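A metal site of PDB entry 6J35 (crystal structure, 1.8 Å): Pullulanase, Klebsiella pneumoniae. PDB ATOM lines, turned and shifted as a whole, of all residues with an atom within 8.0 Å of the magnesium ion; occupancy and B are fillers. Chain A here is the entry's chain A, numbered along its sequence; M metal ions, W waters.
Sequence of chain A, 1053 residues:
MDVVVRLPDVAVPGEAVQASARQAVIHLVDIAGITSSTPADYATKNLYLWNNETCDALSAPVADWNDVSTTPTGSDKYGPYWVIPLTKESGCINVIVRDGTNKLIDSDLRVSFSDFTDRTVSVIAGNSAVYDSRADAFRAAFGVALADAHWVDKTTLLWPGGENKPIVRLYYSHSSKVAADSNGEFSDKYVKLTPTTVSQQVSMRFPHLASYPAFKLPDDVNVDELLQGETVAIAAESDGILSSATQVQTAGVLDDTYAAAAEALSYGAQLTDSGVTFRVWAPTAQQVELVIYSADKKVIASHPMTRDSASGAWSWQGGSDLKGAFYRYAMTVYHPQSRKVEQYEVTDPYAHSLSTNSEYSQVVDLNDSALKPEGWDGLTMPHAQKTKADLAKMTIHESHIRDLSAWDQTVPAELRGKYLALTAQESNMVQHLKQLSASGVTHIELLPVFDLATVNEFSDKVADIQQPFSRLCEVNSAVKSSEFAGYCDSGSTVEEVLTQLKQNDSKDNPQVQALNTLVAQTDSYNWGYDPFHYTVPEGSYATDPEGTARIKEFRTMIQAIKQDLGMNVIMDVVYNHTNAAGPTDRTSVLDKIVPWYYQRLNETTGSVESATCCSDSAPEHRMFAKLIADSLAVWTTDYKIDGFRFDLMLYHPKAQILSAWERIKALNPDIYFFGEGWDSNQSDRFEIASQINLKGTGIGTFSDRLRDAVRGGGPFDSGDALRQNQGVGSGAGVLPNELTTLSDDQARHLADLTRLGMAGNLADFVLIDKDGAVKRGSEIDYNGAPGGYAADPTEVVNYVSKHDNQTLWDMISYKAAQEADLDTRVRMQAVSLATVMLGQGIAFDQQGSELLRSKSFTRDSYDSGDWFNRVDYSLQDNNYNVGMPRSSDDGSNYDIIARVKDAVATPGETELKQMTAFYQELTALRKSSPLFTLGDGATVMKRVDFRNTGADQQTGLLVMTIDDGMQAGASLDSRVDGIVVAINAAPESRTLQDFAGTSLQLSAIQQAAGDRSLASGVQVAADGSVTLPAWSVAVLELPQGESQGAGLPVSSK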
ATOM      1  N   SER A 929     -28.469 -14.782 -12.312  1.00  0.00           N
ATOM      2  CA  SER A 929     -28.177 -14.310 -10.944  1.00  0.00           C
ATOM      3  C   SER A 929     -29.267 -14.755  -9.982  1.00  0.00           C
ATOM      4  O   SER A 929     -30.461 -14.663 -10.303  1.00  0.00           O
ATOM      5  CB  SER A 929     -28.055 -12.785 -10.879  1.00  0.00           C
ATOM      6  OG  SER A 929     -27.848 -12.341  -9.541  1.00  0.00           O
ATOM      7  N   PRO A 930     -28.899 -15.221  -8.792  1.00  0.00           N
ATOM      8  CA  PRO A 930     -29.904 -15.514  -7.763  1.00  0.00           C
ATOM      9  C   PRO A 930     -30.662 -14.298  -7.243  1.00  0.00           C
ATOM     10  O   PRO A 930     -31.660 -14.475  -6.524  1.00  0.00           O
ATOM     11  CB  PRO A 930     -29.067 -16.156  -6.639  1.00  0.00           C
ATOM     12  CG  PRO A 930     -27.707 -15.599  -6.808  1.00  0.00           C
ATOM     13  CD  PRO A 930     -27.527 -15.522  -8.325  1.00  0.00           C
ATOM     14  N   LEU A 931     -30.210 -13.072  -7.533  1.00  0.00           N
ATOM     15  CA  LEU A 931     -30.954 -11.911  -7.048  1.00  0.00           C
ATOM     16  C   LEU A 931     -32.321 -11.789  -7.733  1.00  0.00           C
ATOM     17  O   LEU A 931     -33.240 -11.187  -7.165  1.00  0.00           O
ATOM     18  CB  LEU A 931     -30.114 -10.637  -7.233  1.00  0.00           C
ATOM     19  CG  LEU A 931     -28.770 -10.648  -6.498  1.00  0.00           C
ATOM     20  CD1 LEU A 931     -27.860  -9.524  -6.981  1.00  0.00           C
ATOM     21  CD2 LEU A 931     -28.978 -10.550  -4.989  1.00  0.00           C
ATOM     22  N   ARG A 943     -34.454  -6.539   0.179  1.00  0.00           N
ATOM     23  CA  ARG A 943     -33.538  -6.276  -0.931  1.00  0.00           C
ATOM     24  C   ARG A 943     -34.159  -5.538  -2.112  1.00  0.00           C
ATOM     25  O   ARG A 943     -33.416  -4.888  -2.851  1.00  0.00           O
ATOM     26  CB  ARG A 943     -32.922  -7.589  -1.443  1.00  0.00           C
ATOM     27  CG  ARG A 943     -32.041  -8.321  -0.431  1.00  0.00           C
ATOM     28  CD  ARG A 943     -31.525  -9.652  -0.998  1.00  0.00           C
ATOM     29  NE  ARG A 943     -30.663 -10.337  -0.035  1.00  0.00           N
ATOM     30  CZ  ARG A 943     -29.344 -10.457  -0.123  1.00  0.00           C
ATOM     31  NH1 ARG A 943     -28.691  -9.970  -1.161  1.00  0.00           N
ATOM     32  NH2 ARG A 943     -28.660 -11.122   0.809  1.00  0.00           N
ATOM     33  N   ASP A 963     -30.880  -5.383  -3.971  1.00  0.00           N
ATOM     34  CA  ASP A 963     -29.664  -5.164  -3.201  1.00  0.00           C
ATOM     35  C   ASP A 963     -28.901  -6.469  -2.989  1.00  0.00           C
ATOM     36  O   ASP A 963     -29.495  -7.487  -2.613  1.00  0.00           O
ATOM     37  CB  ASP A 963     -30.055  -4.550  -1.855  1.00  0.00           C
ATOM     38  CG  ASP A 963     -28.881  -3.978  -1.092  1.00  0.00           C
ATOM     39  OD1 ASP A 963     -27.769  -3.854  -1.659  1.00  0.00           O
ATOM     40  OD2 ASP A 963     -29.109  -3.644   0.095  1.00  0.00           O
ATOM     41  N   ASP A 964     -27.588  -6.446  -3.233  1.00  0.00           N
ATOM     42  CA  ASP A 964     -26.715  -7.498  -2.729  1.00  0.00           C
ATOM     43  C   ASP A 964     -25.629  -6.946  -1.795  1.00  0.00           C
ATOM     44  O   ASP A 964     -24.656  -7.660  -1.510  1.00  0.00           O
ATOM     45  CB  ASP A 964     -26.065  -8.296  -3.867  1.00  0.00           C
ATOM     46  CG  ASP A 964     -25.720  -9.733  -3.459  1.00  0.00           C
ATOM     47  OD1 ASP A 964     -26.460 -10.320  -2.634  1.00  0.00           O
ATOM     48  OD2 ASP A 964     -24.692 -10.280  -3.944  1.00  0.00           O
ATOM     49  N   GLY A 965     -25.775  -5.692  -1.335  1.00  0.00           N
ATOM     50  CA  GLY A 965     -24.760  -5.066  -0.506  1.00  0.00           C
ATOM     51  C   GLY A 965     -24.916  -5.333   0.986  1.00  0.00           C
ATOM     52  O   GLY A 965     -25.813  -6.037   1.453  1.00  0.00           O
ATOM     53  N   ALA A 970     -25.891 -11.223   3.447  1.00  0.00           N
ATOM     54  CA  ALA A 970     -24.757 -11.808   2.763  1.00  0.00           C
ATOM     55  C   ALA A 970     -24.842 -11.564   1.266  1.00  0.00           C
ATOM     56  O   ALA A 970     -25.918 -11.346   0.707  1.00  0.00           O
ATOM     57  CB  ALA A 970     -24.684 -13.315   3.047  1.00  0.00           C
ATOM     58  N   SER A 971     -23.693 -11.606   0.614  1.00  0.00           N
ATOM     59  CA  SER A 971     -23.664 -11.565  -0.847  1.00  0.00           C
ATOM     60  C   SER A 971     -24.155 -12.902  -1.388  1.00  0.00           C
ATOM     61  O   SER A 971     -23.582 -13.948  -1.090  1.00  0.00           O
ATOM     62  CB  SER A 971     -22.236 -11.273  -1.329  1.00  0.00           C
ATOM     63  OG  SER A 971     -22.097 -11.434  -2.732  1.00  0.00           O
ATOM     64  N   LEU A 972     -25.244 -12.857  -2.159  1.00  0.00           N
ATOM     65  CA  LEU A 972     -25.780 -14.042  -2.815  1.00  0.00           C
ATOM     66  C   LEU A 972     -25.161 -14.278  -4.180  1.00  0.00           C
ATOM     67  O   LEU A 972     -25.326 -15.375  -4.728  1.00  0.00           O
ATOM     68  CB  LEU A 972     -27.292 -13.901  -2.963  1.00  0.00           C
ATOM     69  CG  LEU A 972     -28.076 -13.653  -1.686  1.00  0.00           C
ATOM     70  CD1 LEU A 972     -29.542 -13.480  -2.056  1.00  0.00           C
ATOM     71  CD2 LEU A 972     -27.889 -14.848  -0.752  1.00  0.00           C
ATOM     72  N   ASP A 973     -24.438 -13.302  -4.708  1.00  0.00           N
ATOM     73  CA  ASP A 973     -23.919 -13.326  -6.068  1.00  0.00           C
ATOM     74  C   ASP A 973     -22.537 -12.690  -5.995  1.00  0.00           C
ATOM     75  O   ASP A 973     -22.428 -11.477  -5.744  1.00  0.00           O
ATOM     76  CB  ASP A 973     -24.864 -12.557  -7.005  1.00  0.00           C
ATOM     77  CG  ASP A 973     -24.445 -12.592  -8.472  1.00  0.00           C
ATOM     78  OD1 ASP A 973     -23.295 -12.960  -8.798  1.00  0.00           O
ATOM     79  OD2 ASP A 973     -25.307 -12.227  -9.306  1.00  0.00           O
ATOM     80  N   SER A 974     -21.484 -13.483  -6.173  1.00  0.00           N
ATOM     81  CA  SER A 974     -20.135 -12.956  -6.002  1.00  0.00           C
ATOM     82  C   SER A 974     -19.736 -11.952  -7.071  1.00  0.00           C
ATOM     83  O   SER A 974     -18.745 -11.230  -6.896  1.00  0.00           O
ATOM     84  CB  SER A 974     -19.126 -14.126  -5.981  1.00  0.00           C
ATOM     85  OG  SER A 974     -19.094 -14.773  -7.236  1.00  0.00           O
ATOM     86  N   ARG A 975     -20.466 -11.884  -8.186  1.00  0.00           N
ATOM     87  CA  ARG A 975     -20.084 -11.001  -9.278  1.00  0.00           C
ATOM     88  C   ARG A 975     -20.606  -9.590  -9.131  1.00  0.00           C
ATOM     89  O   ARG A 975     -20.024  -8.681  -9.717  1.00  0.00           O
ATOM     90  CB  ARG A 975     -20.568 -11.574 -10.616  1.00  0.00           C
ATOM     91  CG  ARG A 975     -19.977 -12.937 -10.924  1.00  0.00           C
ATOM     92  CD  ARG A 975     -20.082 -13.308 -12.383  1.00  0.00           C
ATOM     93  NE  ARG A 975     -19.603 -14.668 -12.625  1.00  0.00           N
ATOM     94  CZ  ARG A 975     -19.561 -15.240 -13.824  1.00  0.00           C
ATOM     95  NH1 ARG A 975     -19.096 -16.478 -13.963  1.00  0.00           N
ATOM     96  NH2 ARG A 975     -19.982 -14.551 -14.902  1.00  0.00           N
ATOM     97  N   VAL A 976     -21.681  -9.364  -8.372  1.00  0.00           N
ATOM     98  CA  VAL A 976     -22.323  -8.055  -8.326  1.00  0.00           C
ATOM     99  C   VAL A 976     -22.726  -7.729  -6.893  1.00  0.00           C
ATOM    100  O   VAL A 976     -22.955  -8.615  -6.065  1.00  0.00           O
ATOM    101  CB  VAL A 976     -23.571  -7.939  -9.236  1.00  0.00           C
ATOM    102  CG1 VAL A 976     -23.265  -8.378 -10.672  1.00  0.00           C
ATOM    103  CG2 VAL A 976     -24.752  -8.717  -8.672  1.00  0.00           C
ATOM    104  N   ASP A 977     -22.847  -6.426  -6.636  1.00  0.00           N
ATOM    105  CA  ASP A 977     -23.338  -5.869  -5.375  1.00  0.00           C
ATOM    106  C   ASP A 977     -24.777  -5.405  -5.479  1.00  0.00           C
ATOM    107  O   ASP A 977     -25.342  -4.924  -4.491  1.00  0.00           O
ATOM    108  CB  ASP A 977     -22.462  -4.691  -4.940  1.00  0.00           C
ATOM    109  CG  ASP A 977     -21.141  -5.132  -4.326  1.00  0.00           C
ATOM    110  OD1 ASP A 977     -21.103  -6.162  -3.617  1.00  0.00           O
ATOM    111  OD2 ASP A 977     -20.129  -4.430  -4.546  1.00  0.00           O
ATOM    112  N   GLY A 978     -25.382  -5.532  -6.642  1.00  0.00           N
ATOM    113  CA  GLY A 978     -26.739  -5.079  -6.829  1.00  0.00           C
ATOM    114  C   GLY A 978     -27.113  -5.083  -8.297  1.00  0.00           C
ATOM    115  O   GLY A 978     -26.233  -5.120  -9.162  1.00  0.00           O
ATOM    116  N   LEU A1038     -23.924  -3.466 -10.289  1.00  0.00           N
ATOM    117  CA  LEU A1038     -22.786  -2.915  -9.587  1.00  0.00           C
ATOM    118  C   LEU A1038     -21.735  -4.005  -9.484  1.00  0.00           C
ATOM    119  O   LEU A1038     -21.959  -4.997  -8.774  1.00  0.00           O
ATOM    120  CB  LEU A1038     -23.201  -2.439  -8.192  1.00  0.00           C
ATOM    121  CG  LEU A1038     -24.197  -1.274  -8.123  1.00  0.00           C
ATOM    122  CD1 LEU A1038     -24.599  -1.014  -6.685  1.00  0.00           C
ATOM    123  CD2 LEU A1038     -23.611  -0.001  -8.766  1.00  0.00           C
ATOM    124  N   PRO A1039     -20.596  -3.899 -10.164  1.00  0.00           N
ATOM    125  CA  PRO A1039     -19.596  -4.974 -10.100  1.00  0.00           C
ATOM    126  C   PRO A1039     -19.051  -5.129  -8.682  1.00  0.00           C
ATOM    127  O   PRO A1039     -18.778  -4.146  -8.003  1.00  0.00           O
ATOM    128  CB  PRO A1039     -18.492  -4.492 -11.057  1.00  0.00           C
ATOM    129  CG  PRO A1039     -18.626  -3.001 -11.038  1.00  0.00           C
ATOM    130  CD  PRO A1039     -20.106  -2.734 -10.925  1.00  0.00           C
ATOM    131  N   GLN A1040     -18.889  -6.388  -8.248  1.00  0.00           N
ATOM    132  CA  GLN A1040     -18.416  -6.637  -6.887  1.00  0.00           C
ATOM    133  C   GLN A1040     -16.894  -6.730  -6.877  1.00  0.00           C
ATOM    134  O   GLN A1040     -16.303  -7.391  -7.743  1.00  0.00           O
ATOM    135  CB  GLN A1040     -19.014  -7.918  -6.316  1.00  0.00           C
ATOM    136  CG  GLN A1040     -18.727  -8.143  -4.827  1.00  0.00           C
ATOM    137  CD  GLN A1040     -19.525  -9.300  -4.260  1.00  0.00           C
ATOM    138  OE1 GLN A1040     -20.621  -9.592  -4.758  1.00  0.00           O
ATOM    139  NE2 GLN A1040     -18.994  -9.970  -3.244  1.00  0.00           N
ATOM    140  N   GLY A1041     -16.275  -6.051  -5.921  1.00  0.00           N
ATOM    141  CA  GLY A1041     -14.828  -5.997  -5.821  1.00  0.00           C
ATOM    142  C   GLY A1041     -14.289  -6.946  -4.773  1.00  0.00           C
ATOM    143  O   GLY A1041     -14.817  -8.043  -4.564  1.00  0.00           O
ATOM    144  N   SER A1043     -14.271  -6.924  -1.489  1.00  0.00           N
ATOM    145  CA  SER A1043     -15.271  -7.287  -0.508  1.00  0.00           C
ATOM    146  C   SER A1043     -16.647  -6.864  -0.989  1.00  0.00           C
ATOM    147  O   SER A1043     -16.787  -6.009  -1.871  1.00  0.00           O
ATOM    148  CB  SER A1043     -14.997  -6.613   0.856  1.00  0.00           C
ATOM    149  OG  SER A1043     -13.642  -6.732   1.230  1.00  0.00           O
ATOM    150  N   GLN A1044     -17.674  -7.439  -0.372  1.00  0.00           N
ATOM    151  CA  GLN A1044     -19.022  -6.957  -0.565  1.00  0.00           C
ATOM    152  C   GLN A1044     -19.086  -5.441  -0.368  1.00  0.00           C
ATOM    153  O   GLN A1044     -18.484  -4.894   0.574  1.00  0.00           O
ATOM    154  CB  GLN A1044     -19.967  -7.677   0.401  1.00  0.00           C
ATOM    155  CG  GLN A1044     -21.416  -7.235   0.326  1.00  0.00           C
ATOM    156  CD  GLN A1044     -22.293  -7.934   1.344  1.00  0.00           C
ATOM    157  OE1 GLN A1044     -21.904  -8.122   2.495  1.00  0.00           O
ATOM    158  NE2 GLN A1044     -23.494  -8.303   0.924  1.00  0.00           N
ATOM    159  N   GLY A1045     -19.805  -4.757  -1.257  1.00  0.00           N
ATOM    160  CA  GLY A1045     -19.887  -3.316  -1.261  1.00  0.00           C
ATOM    161  C   GLY A1045     -21.201  -2.769  -0.735  1.00  0.00           C
ATOM    162  O   GLY A1045     -22.007  -3.464  -0.119  1.00  0.00           O
HETATM  163 MG    MG M   1     -22.666  -9.929  -4.374  1.00  0.00          MG
HETATM  164  O   HOH W   1     -22.497  -8.360  -2.992  1.00  0.00           O
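OD2 of Asp 973 sits at hydrogen-bond distance from OG of Ser 929 (2.6 Å). O of Asp 977 is in hydrogen-bond range of N of Asp 964, 3.0 Å away. N of Leu 972 lies within hydrogen-bond range of OD1 of Asp 964, 2.9 Å away. NE2 of Gln 1044 is in hydrogen-bond range of O of Asp 964 (2.8 Å). The side-chain carboxylate of Asp 964 lies within salt-bridge range of the guanidinium group of Arg 943 (2.7 Å). O of Ser 974 lies close to OE1 of Gln 1040, 3.3 Å away. O of Arg 975 lies within hydrogen-bond range of N of Gln 1040 (3.0 Å). NE2 of Gln 1044 lies close to N of Ser 971.
The magnesium ion is bound by O of Asp 973 (2.1 Å), water W1 (2.1 Å), OD2 of Asp 964 (2.1 Å), OE1 of Gln 1040 (2.1 Å), O of Val 976 (2.2 Å) and OG of Ser 971 (2.3 Å). The magnesium ion has six donor atoms within binding distance.
Within 4 Å of the magnesium ion: Asp 964, Ser 971, Asp 973, Val 976 and Gln 1040.
Water W1 bridges the side-chain carboxylate of Asp 977 and the backbone carbonyl oxygen of Asp 964.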
